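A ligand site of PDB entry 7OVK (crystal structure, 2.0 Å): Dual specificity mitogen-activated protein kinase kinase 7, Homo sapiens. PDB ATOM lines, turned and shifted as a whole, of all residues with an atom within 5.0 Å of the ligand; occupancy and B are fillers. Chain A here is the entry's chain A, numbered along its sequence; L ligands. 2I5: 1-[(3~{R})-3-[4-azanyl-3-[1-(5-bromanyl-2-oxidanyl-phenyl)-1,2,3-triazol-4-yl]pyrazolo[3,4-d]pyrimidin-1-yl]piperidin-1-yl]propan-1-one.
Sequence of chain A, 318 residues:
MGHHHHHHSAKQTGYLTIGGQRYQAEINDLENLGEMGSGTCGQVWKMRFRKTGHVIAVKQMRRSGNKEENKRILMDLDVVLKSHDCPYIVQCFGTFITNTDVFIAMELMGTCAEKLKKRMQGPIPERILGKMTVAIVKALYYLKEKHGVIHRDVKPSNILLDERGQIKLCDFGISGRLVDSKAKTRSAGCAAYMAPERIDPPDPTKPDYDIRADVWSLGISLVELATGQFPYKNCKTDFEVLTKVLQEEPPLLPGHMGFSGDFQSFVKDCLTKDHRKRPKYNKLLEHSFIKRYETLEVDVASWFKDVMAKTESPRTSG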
ATOM      1  N   MET A  36     -18.726  10.988  27.643  1.00  0.00           N
ATOM      2  CA  MET A  36     -18.351   9.673  28.144  1.00  0.00           C
ATOM      3  C   MET A  36     -17.144   9.087  27.424  1.00  0.00           C
ATOM      4  O   MET A  36     -16.526   8.160  27.942  1.00  0.00           O
ATOM      5  CB  MET A  36     -19.533   8.706  28.030  1.00  0.00           C
ATOM      6  CG  MET A  36     -20.780   9.176  28.745  1.00  0.00           C
ATOM      7  SD  MET A  36     -21.998   7.863  28.927  1.00  0.00           S
ATOM      8  CE  MET A  36     -22.209   7.345  27.235  1.00  0.00           C
ATOM      9  N   GLY A  37     -16.803   9.625  26.250  1.00  0.00           N
ATOM     10  CA  GLY A  37     -15.689   9.134  25.462  1.00  0.00           C
ATOM     11  C   GLY A  37     -14.338   9.216  26.148  1.00  0.00           C
ATOM     12  O   GLY A  37     -13.333   8.763  25.607  1.00  0.00           O
ATOM     13  N   VAL A  44     -20.104  10.847  22.398  1.00  0.00           N
ATOM     14  CA  VAL A  44     -21.236  10.265  23.101  1.00  0.00           C
ATOM     15  C   VAL A  44     -21.368  10.957  24.452  1.00  0.00           C
ATOM     16  O   VAL A  44     -20.446  10.894  25.272  1.00  0.00           O
ATOM     17  CB  VAL A  44     -21.087   8.742  23.280  1.00  0.00           C
ATOM     18  CG1 VAL A  44     -22.403   8.137  23.742  1.00  0.00           C
ATOM     19  CG2 VAL A  44     -20.618   8.098  21.973  1.00  0.00           C
ATOM     20  N   ALA A  57     -27.717   7.926  27.199  1.00  0.00           N
ATOM     21  CA  ALA A  57     -26.551   8.179  26.358  1.00  0.00           C
ATOM     22  C   ALA A  57     -27.019   8.791  25.049  1.00  0.00           C
ATOM     23  O   ALA A  57     -28.011   8.357  24.461  1.00  0.00           O
ATOM     24  CB  ALA A  57     -25.764   6.901  26.087  1.00  0.00           C
ATOM     25  N   LYS A  59     -25.578  10.103  21.286  1.00  0.00           N
ATOM     26  CA  LYS A  59     -24.543  10.194  20.270  1.00  0.00           C
ATOM     27  C   LYS A  59     -24.880  11.342  19.334  1.00  0.00           C
ATOM     28  O   LYS A  59     -25.996  11.415  18.803  1.00  0.00           O
ATOM     29  CB  LYS A  59     -24.412   8.884  19.488  1.00  0.00           C
ATOM     30  CG  LYS A  59     -23.259   8.857  18.485  1.00  0.00           C
ATOM     31  CD  LYS A  59     -23.088   7.469  17.872  1.00  0.00           C
ATOM     32  CE  LYS A  59     -21.927   7.438  16.884  1.00  0.00           C
ATOM     33  NZ  LYS A  59     -20.637   7.849  17.507  1.00  0.00           N
ATOM     34  N   ILE A  73     -22.152   5.895  10.910  1.00  0.00           N
ATOM     35  CA  ILE A  73     -23.120   6.122  11.978  1.00  0.00           C
ATOM     36  C   ILE A  73     -24.535   5.835  11.488  1.00  0.00           C
ATOM     37  O   ILE A  73     -25.335   5.202  12.187  1.00  0.00           O
ATOM     38  CB  ILE A  73     -22.992   7.554  12.527  1.00  0.00           C
ATOM     39  CG1 ILE A  73     -21.657   7.725  13.264  1.00  0.00           C
ATOM     40  CG2 ILE A  73     -24.153   7.880  13.444  1.00  0.00           C
ATOM     41  CD1 ILE A  73     -21.360   9.157  13.658  1.00  0.00           C
ATOM     42  N   ASP A  76     -25.183   1.992  11.106  1.00  0.00           N
ATOM     43  CA  ASP A  76     -25.397   1.335  12.389  1.00  0.00           C
ATOM     44  C   ASP A  76     -26.742   1.722  12.991  1.00  0.00           C
ATOM     45  O   ASP A  76     -27.430   0.873  13.575  1.00  0.00           O
ATOM     46  CB  ASP A  76     -24.268   1.691  13.355  1.00  0.00           C
ATOM     47  CG  ASP A  76     -22.921   1.149  12.905  1.00  0.00           C
ATOM     48  OD1 ASP A  76     -22.897   0.340  11.951  1.00  0.00           O
ATOM     49  OD2 ASP A  76     -21.890   1.531  13.505  1.00  0.00           O
ATOM     50  N   LEU A  77     -27.131   2.992  12.866  1.00  0.00           N
ATOM     51  CA  LEU A  77     -28.435   3.412  13.371  1.00  0.00           C
ATOM     52  C   LEU A  77     -29.566   2.684  12.662  1.00  0.00           C
ATOM     53  O   LEU A  77     -30.576   2.345  13.280  1.00  0.00           O
ATOM     54  CB  LEU A  77     -28.596   4.932  13.204  1.00  0.00           C
ATOM     55  CG  LEU A  77     -29.955   5.505  13.587  1.00  0.00           C
ATOM     56  CD1 LEU A  77     -30.248   5.293  15.063  1.00  0.00           C
ATOM     57  CD2 LEU A  77     -30.025   6.992  13.239  1.00  0.00           C
ATOM     58  N   VAL A  80     -29.726  -0.609  14.358  1.00  0.00           N
ATOM     59  CA  VAL A  80     -30.166  -0.471  15.737  1.00  0.00           C
ATOM     60  C   VAL A  80     -31.672  -0.228  15.799  1.00  0.00           C
ATOM     61  O   VAL A  80     -32.370  -0.769  16.666  1.00  0.00           O
ATOM     62  CB  VAL A  80     -29.374   0.652  16.441  1.00  0.00           C
ATOM     63  CG1 VAL A  80     -30.019   1.001  17.776  1.00  0.00           C
ATOM     64  CG2 VAL A  80     -27.932   0.228  16.656  1.00  0.00           C
ATOM     65  N   VAL A  90     -27.673  -2.840  22.234  1.00  0.00           N
ATOM     66  CA  VAL A  90     -28.043  -1.585  22.894  1.00  0.00           C
ATOM     67  C   VAL A  90     -29.155  -0.916  22.111  1.00  0.00           C
ATOM     68  O   VAL A  90     -29.102  -0.813  20.873  1.00  0.00           O
ATOM     69  CB  VAL A  90     -26.804  -0.675  23.037  1.00  0.00           C
ATOM     70  CG1 VAL A  90     -25.862  -1.233  24.085  1.00  0.00           C
ATOM     71  CG2 VAL A  90     -26.087  -0.544  21.715  1.00  0.00           C
ATOM     72  N   ILE A 104     -28.749  11.014  18.736  1.00  0.00           N
ATOM     73  CA  ILE A 104     -29.273   9.652  18.826  1.00  0.00           C
ATOM     74  C   ILE A 104     -29.285   9.251  20.294  1.00  0.00           C
ATOM     75  O   ILE A 104     -28.231   9.114  20.927  1.00  0.00           O
ATOM     76  CB  ILE A 104     -28.419   8.669  18.000  1.00  0.00           C
ATOM     77  CG1 ILE A 104     -28.280   9.160  16.562  1.00  0.00           C
ATOM     78  CG2 ILE A 104     -29.038   7.273  18.040  1.00  0.00           C
ATOM     79  CD1 ILE A 104     -27.303   8.363  15.731  1.00  0.00           C
ATOM     80  N   MET A 106     -29.574   6.718  23.161  1.00  0.00           N
ATOM     81  CA  MET A 106     -29.373   5.299  23.424  1.00  0.00           C
ATOM     82  C   MET A 106     -29.546   5.022  24.905  1.00  0.00           C
ATOM     83  O   MET A 106     -29.436   5.929  25.745  1.00  0.00           O
ATOM     84  CB  MET A 106     -27.975   4.845  22.973  1.00  0.00           C
ATOM     85  CG  MET A 106     -27.644   5.162  21.521  1.00  0.00           C
ATOM     86  SD  MET A 106     -28.552   4.140  20.345  1.00  0.00           S
ATOM     87  CE  MET A 106     -27.995   2.507  20.823  1.00  0.00           C
ATOM     88  N   GLU A 107     -29.836   3.764  25.240  1.00  0.00           N
ATOM     89  CA  GLU A 107     -29.910   3.372  26.637  1.00  0.00           C
ATOM     90  C   GLU A 107     -28.534   3.474  27.280  1.00  0.00           C
ATOM     91  O   GLU A 107     -27.521   3.101  26.679  1.00  0.00           O
ATOM     92  CB  GLU A 107     -30.470   1.961  26.776  1.00  0.00           C
ATOM     93  CG  GLU A 107     -29.676   0.855  26.109  1.00  0.00           C
ATOM     94  CD  GLU A 107     -30.250  -0.524  26.380  1.00  0.00           C
ATOM     95  OE1 GLU A 107     -30.764  -0.754  27.502  1.00  0.00           O
ATOM     96  OE2 GLU A 107     -30.211  -1.380  25.468  1.00  0.00           O
ATOM     97  N   LEU A 108     -28.490   3.991  28.497  1.00  0.00           N
ATOM     98  CA  LEU A 108     -27.229   4.232  29.184  1.00  0.00           C
ATOM     99  C   LEU A 108     -26.728   2.929  29.821  1.00  0.00           C
ATOM    100  O   LEU A 108     -27.334   2.428  30.768  1.00  0.00           O
ATOM    101  CB  LEU A 108     -27.394   5.315  30.250  1.00  0.00           C
ATOM    102  CG  LEU A 108     -26.107   5.698  30.984  1.00  0.00           C
ATOM    103  CD1 LEU A 108     -25.158   6.432  30.041  1.00  0.00           C
ATOM    104  CD2 LEU A 108     -26.396   6.523  32.226  1.00  0.00           C
ATOM    105  N   MET A 109     -25.643   2.380  29.287  1.00  0.00           N
ATOM    106  CA  MET A 109     -24.988   1.253  29.906  1.00  0.00           C
ATOM    107  C   MET A 109     -23.943   1.744  30.911  1.00  0.00           C
ATOM    108  O   MET A 109     -23.619   2.932  30.973  1.00  0.00           O
ATOM    109  CB  MET A 109     -24.328   0.355  28.843  1.00  0.00           C
ATOM    110  CG  MET A 109     -25.274  -0.152  27.765  1.00  0.00           C
ATOM    111  SD  MET A 109     -26.491  -1.327  28.380  1.00  0.00           S
ATOM    112  CE  MET A 109     -25.459  -2.745  28.770  1.00  0.00           C
ATOM    113  N   GLY A 110     -23.428   0.816  31.711  1.00  0.00           N
ATOM    114  CA  GLY A 110     -22.424   1.155  32.709  1.00  0.00           C
ATOM    115  C   GLY A 110     -21.063   1.427  32.101  1.00  0.00           C
ATOM    116  O   GLY A 110     -20.606   2.573  32.051  1.00  0.00           O
ATOM    117  N   THR A 111     -20.403   0.369  31.637  1.00  0.00           N
ATOM    118  CA  THR A 111     -19.100   0.487  30.997  1.00  0.00           C
ATOM    119  C   THR A 111     -18.881  -0.770  30.158  1.00  0.00           C
ATOM    120  O   THR A 111     -19.746  -1.648  30.096  1.00  0.00           O
ATOM    121  CB  THR A 111     -17.969   0.669  32.021  1.00  0.00           C
ATOM    122  OG1 THR A 111     -16.749   0.986  31.335  1.00  0.00           O
ATOM    123  CG2 THR A 111     -17.770  -0.598  32.837  1.00  0.00           C
ATOM    124  N   CYS A 112     -17.722  -0.855  29.531  1.00  0.00           N
ATOM    125  CA  CYS A 112     -17.405  -1.973  28.643  1.00  0.00           C
ATOM    126  C   CYS A 112     -16.486  -2.974  29.333  1.00  0.00           C
ATOM    127  O   CYS A 112     -15.923  -2.713  30.399  1.00  0.00           O
ATOM    128  CB  CYS A 112     -16.769  -1.471  27.348  1.00  0.00           C
ATOM    129  SG  CYS A 112     -15.178  -0.682  27.568  1.00  0.00           S
ATOM    130  N   GLU A 114     -13.574  -3.960  28.468  1.00  0.00           N
ATOM    131  CA  GLU A 114     -12.190  -3.510  28.540  1.00  0.00           C
ATOM    132  C   GLU A 114     -11.930  -2.727  29.821  1.00  0.00           C
ATOM    133  O   GLU A 114     -10.900  -2.906  30.477  1.00  0.00           O
ATOM    134  CB  GLU A 114     -11.841  -2.662  27.322  1.00  0.00           C
ATOM    135  CG  GLU A 114     -10.369  -2.314  27.231  1.00  0.00           C
ATOM    136  CD  GLU A 114     -10.064  -1.418  26.049  1.00  0.00           C
ATOM    137  OE1 GLU A 114     -10.651  -0.316  25.968  1.00  0.00           O
ATOM    138  OE2 GLU A 114      -9.254  -1.833  25.193  1.00  0.00           O
ATOM    139  N   LYS A 115     -12.862  -1.834  30.190  1.00  0.00           N
ATOM    140  CA  LYS A 115     -12.696  -1.053  31.415  1.00  0.00           C
ATOM    141  C   LYS A 115     -12.886  -1.925  32.654  1.00  0.00           C
ATOM    142  O   LYS A 115     -12.206  -1.728  33.665  1.00  0.00           O
ATOM    143  CB  LYS A 115     -13.676   0.111  31.429  1.00  0.00           C
ATOM    144  CG  LYS A 115     -13.664   0.943  30.159  1.00  0.00           C
ATOM    145  CD  LYS A 115     -12.347   1.671  29.963  1.00  0.00           C
ATOM    146  CE  LYS A 115     -12.486   3.145  30.294  1.00  0.00           C
ATOM    147  NZ  LYS A 115     -11.159   3.824  30.352  1.00  0.00           N
ATOM    148  N   PRO A 156     -13.318  -6.561  23.661  1.00  0.00           N
ATOM    149  CA  PRO A 156     -13.829  -6.109  24.973  1.00  0.00           C
ATOM    150  C   PRO A 156     -14.364  -4.687  24.987  1.00  0.00           C
ATOM    151  O   PRO A 156     -15.214  -4.372  25.827  1.00  0.00           O
ATOM    152  CB  PRO A 156     -12.606  -6.252  25.874  1.00  0.00           C
ATOM    153  CG  PRO A 156     -11.830  -7.361  25.277  1.00  0.00           C
ATOM    154  CD  PRO A 156     -12.009  -7.214  23.788  1.00  0.00           C
ATOM    155  N   SER A 157     -13.902  -3.822  24.087  1.00  0.00           N
ATOM    156  CA  SER A 157     -14.409  -2.455  24.032  1.00  0.00           C
ATOM    157  C   SER A 157     -15.783  -2.350  23.383  1.00  0.00           C
ATOM    158  O   SER A 157     -16.407  -1.287  23.449  1.00  0.00           O
ATOM    159  CB  SER A 157     -13.411  -1.560  23.291  1.00  0.00           C
ATOM    160  OG  SER A 157     -13.190  -2.022  21.964  1.00  0.00           O
ATOM    161  N   LEU A 160     -20.779  -4.165  26.254  1.00  0.00           N
ATOM    162  CA  LEU A 160     -21.214  -3.240  27.291  1.00  0.00           C
ATOM    163  C   LEU A 160     -21.990  -3.970  28.380  1.00  0.00           C
ATOM    164  O   LEU A 160     -22.740  -4.916  28.101  1.00  0.00           O
ATOM    165  CB  LEU A 160     -22.084  -2.131  26.694  1.00  0.00           C
ATOM    166  CG  LEU A 160     -21.474  -1.293  25.569  1.00  0.00           C
ATOM    167  CD1 LEU A 160     -22.390  -0.126  25.202  1.00  0.00           C
ATOM    168  CD2 LEU A 160     -20.094  -0.781  25.943  1.00  0.00           C
ATOM    169  N   CYS A 170     -22.433  -3.331  21.028  1.00  0.00           N
ATOM    170  CA  CYS A 170     -22.568  -1.999  20.449  1.00  0.00           C
ATOM    171  C   CYS A 170     -21.544  -1.816  19.353  1.00  0.00           C
ATOM    172  O   CYS A 170     -20.553  -2.559  19.265  1.00  0.00           O
ATOM    173  CB  CYS A 170     -22.421  -0.898  21.504  1.00  0.00           C
ATOM    174  SG  CYS A 170     -20.710  -0.533  21.968  1.00  0.00           S
ATOM    175  N   ASP A 171     -21.781  -0.811  18.502  1.00  0.00           N
ATOM    176  CA  ASP A 171     -20.860  -0.412  17.441  1.00  0.00           C
ATOM    177  C   ASP A 171     -20.577  -1.575  16.495  1.00  0.00           C
ATOM    178  O   ASP A 171     -19.596  -2.313  16.671  1.00  0.00           O
ATOM    179  CB  ASP A 171     -19.569   0.137  18.064  1.00  0.00           C
ATOM    180  CG  ASP A 171     -18.842   1.100  17.147  1.00  0.00           C
ATOM    181  OD1 ASP A 171     -19.495   2.016  16.584  1.00  0.00           O
ATOM    182  OD2 ASP A 171     -17.616   0.957  16.983  1.00  0.00           O
HETATM  183  C10 2I5 L   1     -22.535   3.775  21.304  1.00  0.00           C
HETATM  184  C13 2I5 L   1     -24.717   3.880  18.423  1.00  0.00           C
HETATM  185  C17 2I5 L   1     -22.462   3.408  16.907  1.00  0.00           C
HETATM  186  C24 2I5 L   1     -19.033   4.411  25.529  1.00  0.00           C
HETATM  187  C26 2I5 L   1     -17.246   6.048  25.239  1.00  0.00           C
HETATM  188  C02 2I5 L   1     -23.819   3.528  25.946  1.00  0.00           C
HETATM  189  C04 2I5 L   1     -22.700   3.804  27.955  1.00  0.00           C
HETATM  190  C06 2I5 L   1     -21.465   3.970  25.990  1.00  0.00           C
HETATM  191  C07 2I5 L   1     -22.598   3.727  25.237  1.00  0.00           C
HETATM  192  C08 2I5 L   1     -22.147   3.770  23.868  1.00  0.00           C
HETATM  193  C09 2I5 L   1     -22.969   3.566  22.610  1.00  0.00           C
HETATM  194  C12 2I5 L   1     -23.524   3.557  19.053  1.00  0.00           C
HETATM  195  C14 2I5 L   1     -24.789   3.970  17.049  1.00  0.00           C
HETATM  196  C16 2I5 L   1     -23.666   3.736  16.284  1.00  0.00           C
HETATM  197  C18 2I5 L   1     -22.390   3.317  18.281  1.00  0.00           C
HETATM  198  C25 2I5 L   1     -18.668   5.724  24.982  1.00  0.00           C
HETATM  199  C27 2I5 L   1     -16.292   4.950  24.762  1.00  0.00           C
HETATM  200  C29 2I5 L   1     -15.750   2.788  26.117  1.00  0.00           C
HETATM  201  C30 2I5 L   1     -16.218   1.445  26.682  1.00  0.00           C
HETATM  202  C31 2I5 L   1     -15.420   0.313  26.067  1.00  0.00           C
HETATM  203  C33 2I5 L   1     -18.088   3.293  25.039  1.00  0.00           C
HETATM  204  N01 2I5 L   1     -25.058   3.277  25.244  1.00  0.00           N
HETATM  205  N03 2I5 L   1     -23.821   3.579  27.273  1.00  0.00           N
HETATM  206  N05 2I5 L   1     -21.541   3.998  27.347  1.00  0.00           N
HETATM  207  N11 2I5 L   1     -23.531   3.477  20.494  1.00  0.00           N
HETATM  208  N20 2I5 L   1     -24.595   3.084  21.231  1.00  0.00           N
HETATM  209  N21 2I5 L   1     -24.234   3.138  22.550  1.00  0.00           N
HETATM  210  N22 2I5 L   1     -20.847   4.010  23.869  1.00  0.00           N
HETATM  211  N23 2I5 L   1     -20.438   4.130  25.131  1.00  0.00           N
HETATM  212  N28 2I5 L   1     -16.662   3.625  25.350  1.00  0.00           N
HETATM  213  O19 2I5 L   1     -21.163   2.988  18.884  1.00  0.00           O
HETATM  214  O32 2I5 L   1     -14.651   3.160  26.298  1.00  0.00           O
HETATM  215 BR15 2I5 L   1     -26.482   4.421  16.216  1.00  0.00          BR
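A carbon (C31) of the ligand is covalently linked to the side-chain sulfur (SG) of Cys 112.
The backbone carbonyl oxygen (O) of Glu 107 sits at hydrogen-bond distance from a nitrogen (N01) of the ligand.
A nitrogen (N03) of the ligand is in hydrogen-bond range of the backbone NH of Met 109.
The side-chain carboxylate (OD1) of Asp 171 sits at hydrogen-bond distance from an oxygen (O19) of the ligand (3.0 Å).
The backbone NH of Lys 115 lies close to the side-chain sulfur of Cys 112, at 3.7 Å.
N of Glu 114 sits close to SG of Cys 112, 3.8 Å away.
The backbone NH (N) of Met 36 lies within hydrogen-bond range of the backbone carbonyl oxygen (O) of Val 44.
The backbone NH of Met 106 sits at hydrogen-bond distance from the backbone carbonyl oxygen of Ala 57.
N of Ile 104 sits at hydrogen-bond distance from O of Lys 59, at 2.8 Å.
Merely in contact with the ligand: Met 36, Gly 37, Ala 57, Lys 59, Asp 76, Leu 77, Val 90, Met 106, Leu 108, Ser 157 and Leu 160.
Hydrophobic or aromatic side chains that line the ligand: Met 36, Ala 57, Leu 77, Val 90, Met 106, Met 109 and Leu 160.
15 residues have an atom within 4 Å of the ligand: Met 36, Gly 37, Ala 57, Lys 59, Asp 76, Leu 77, Val 90, Met 106, Glu 107, Leu 108, Met 109, Cys 112, Ser 157, Leu 160 and Asp 171.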
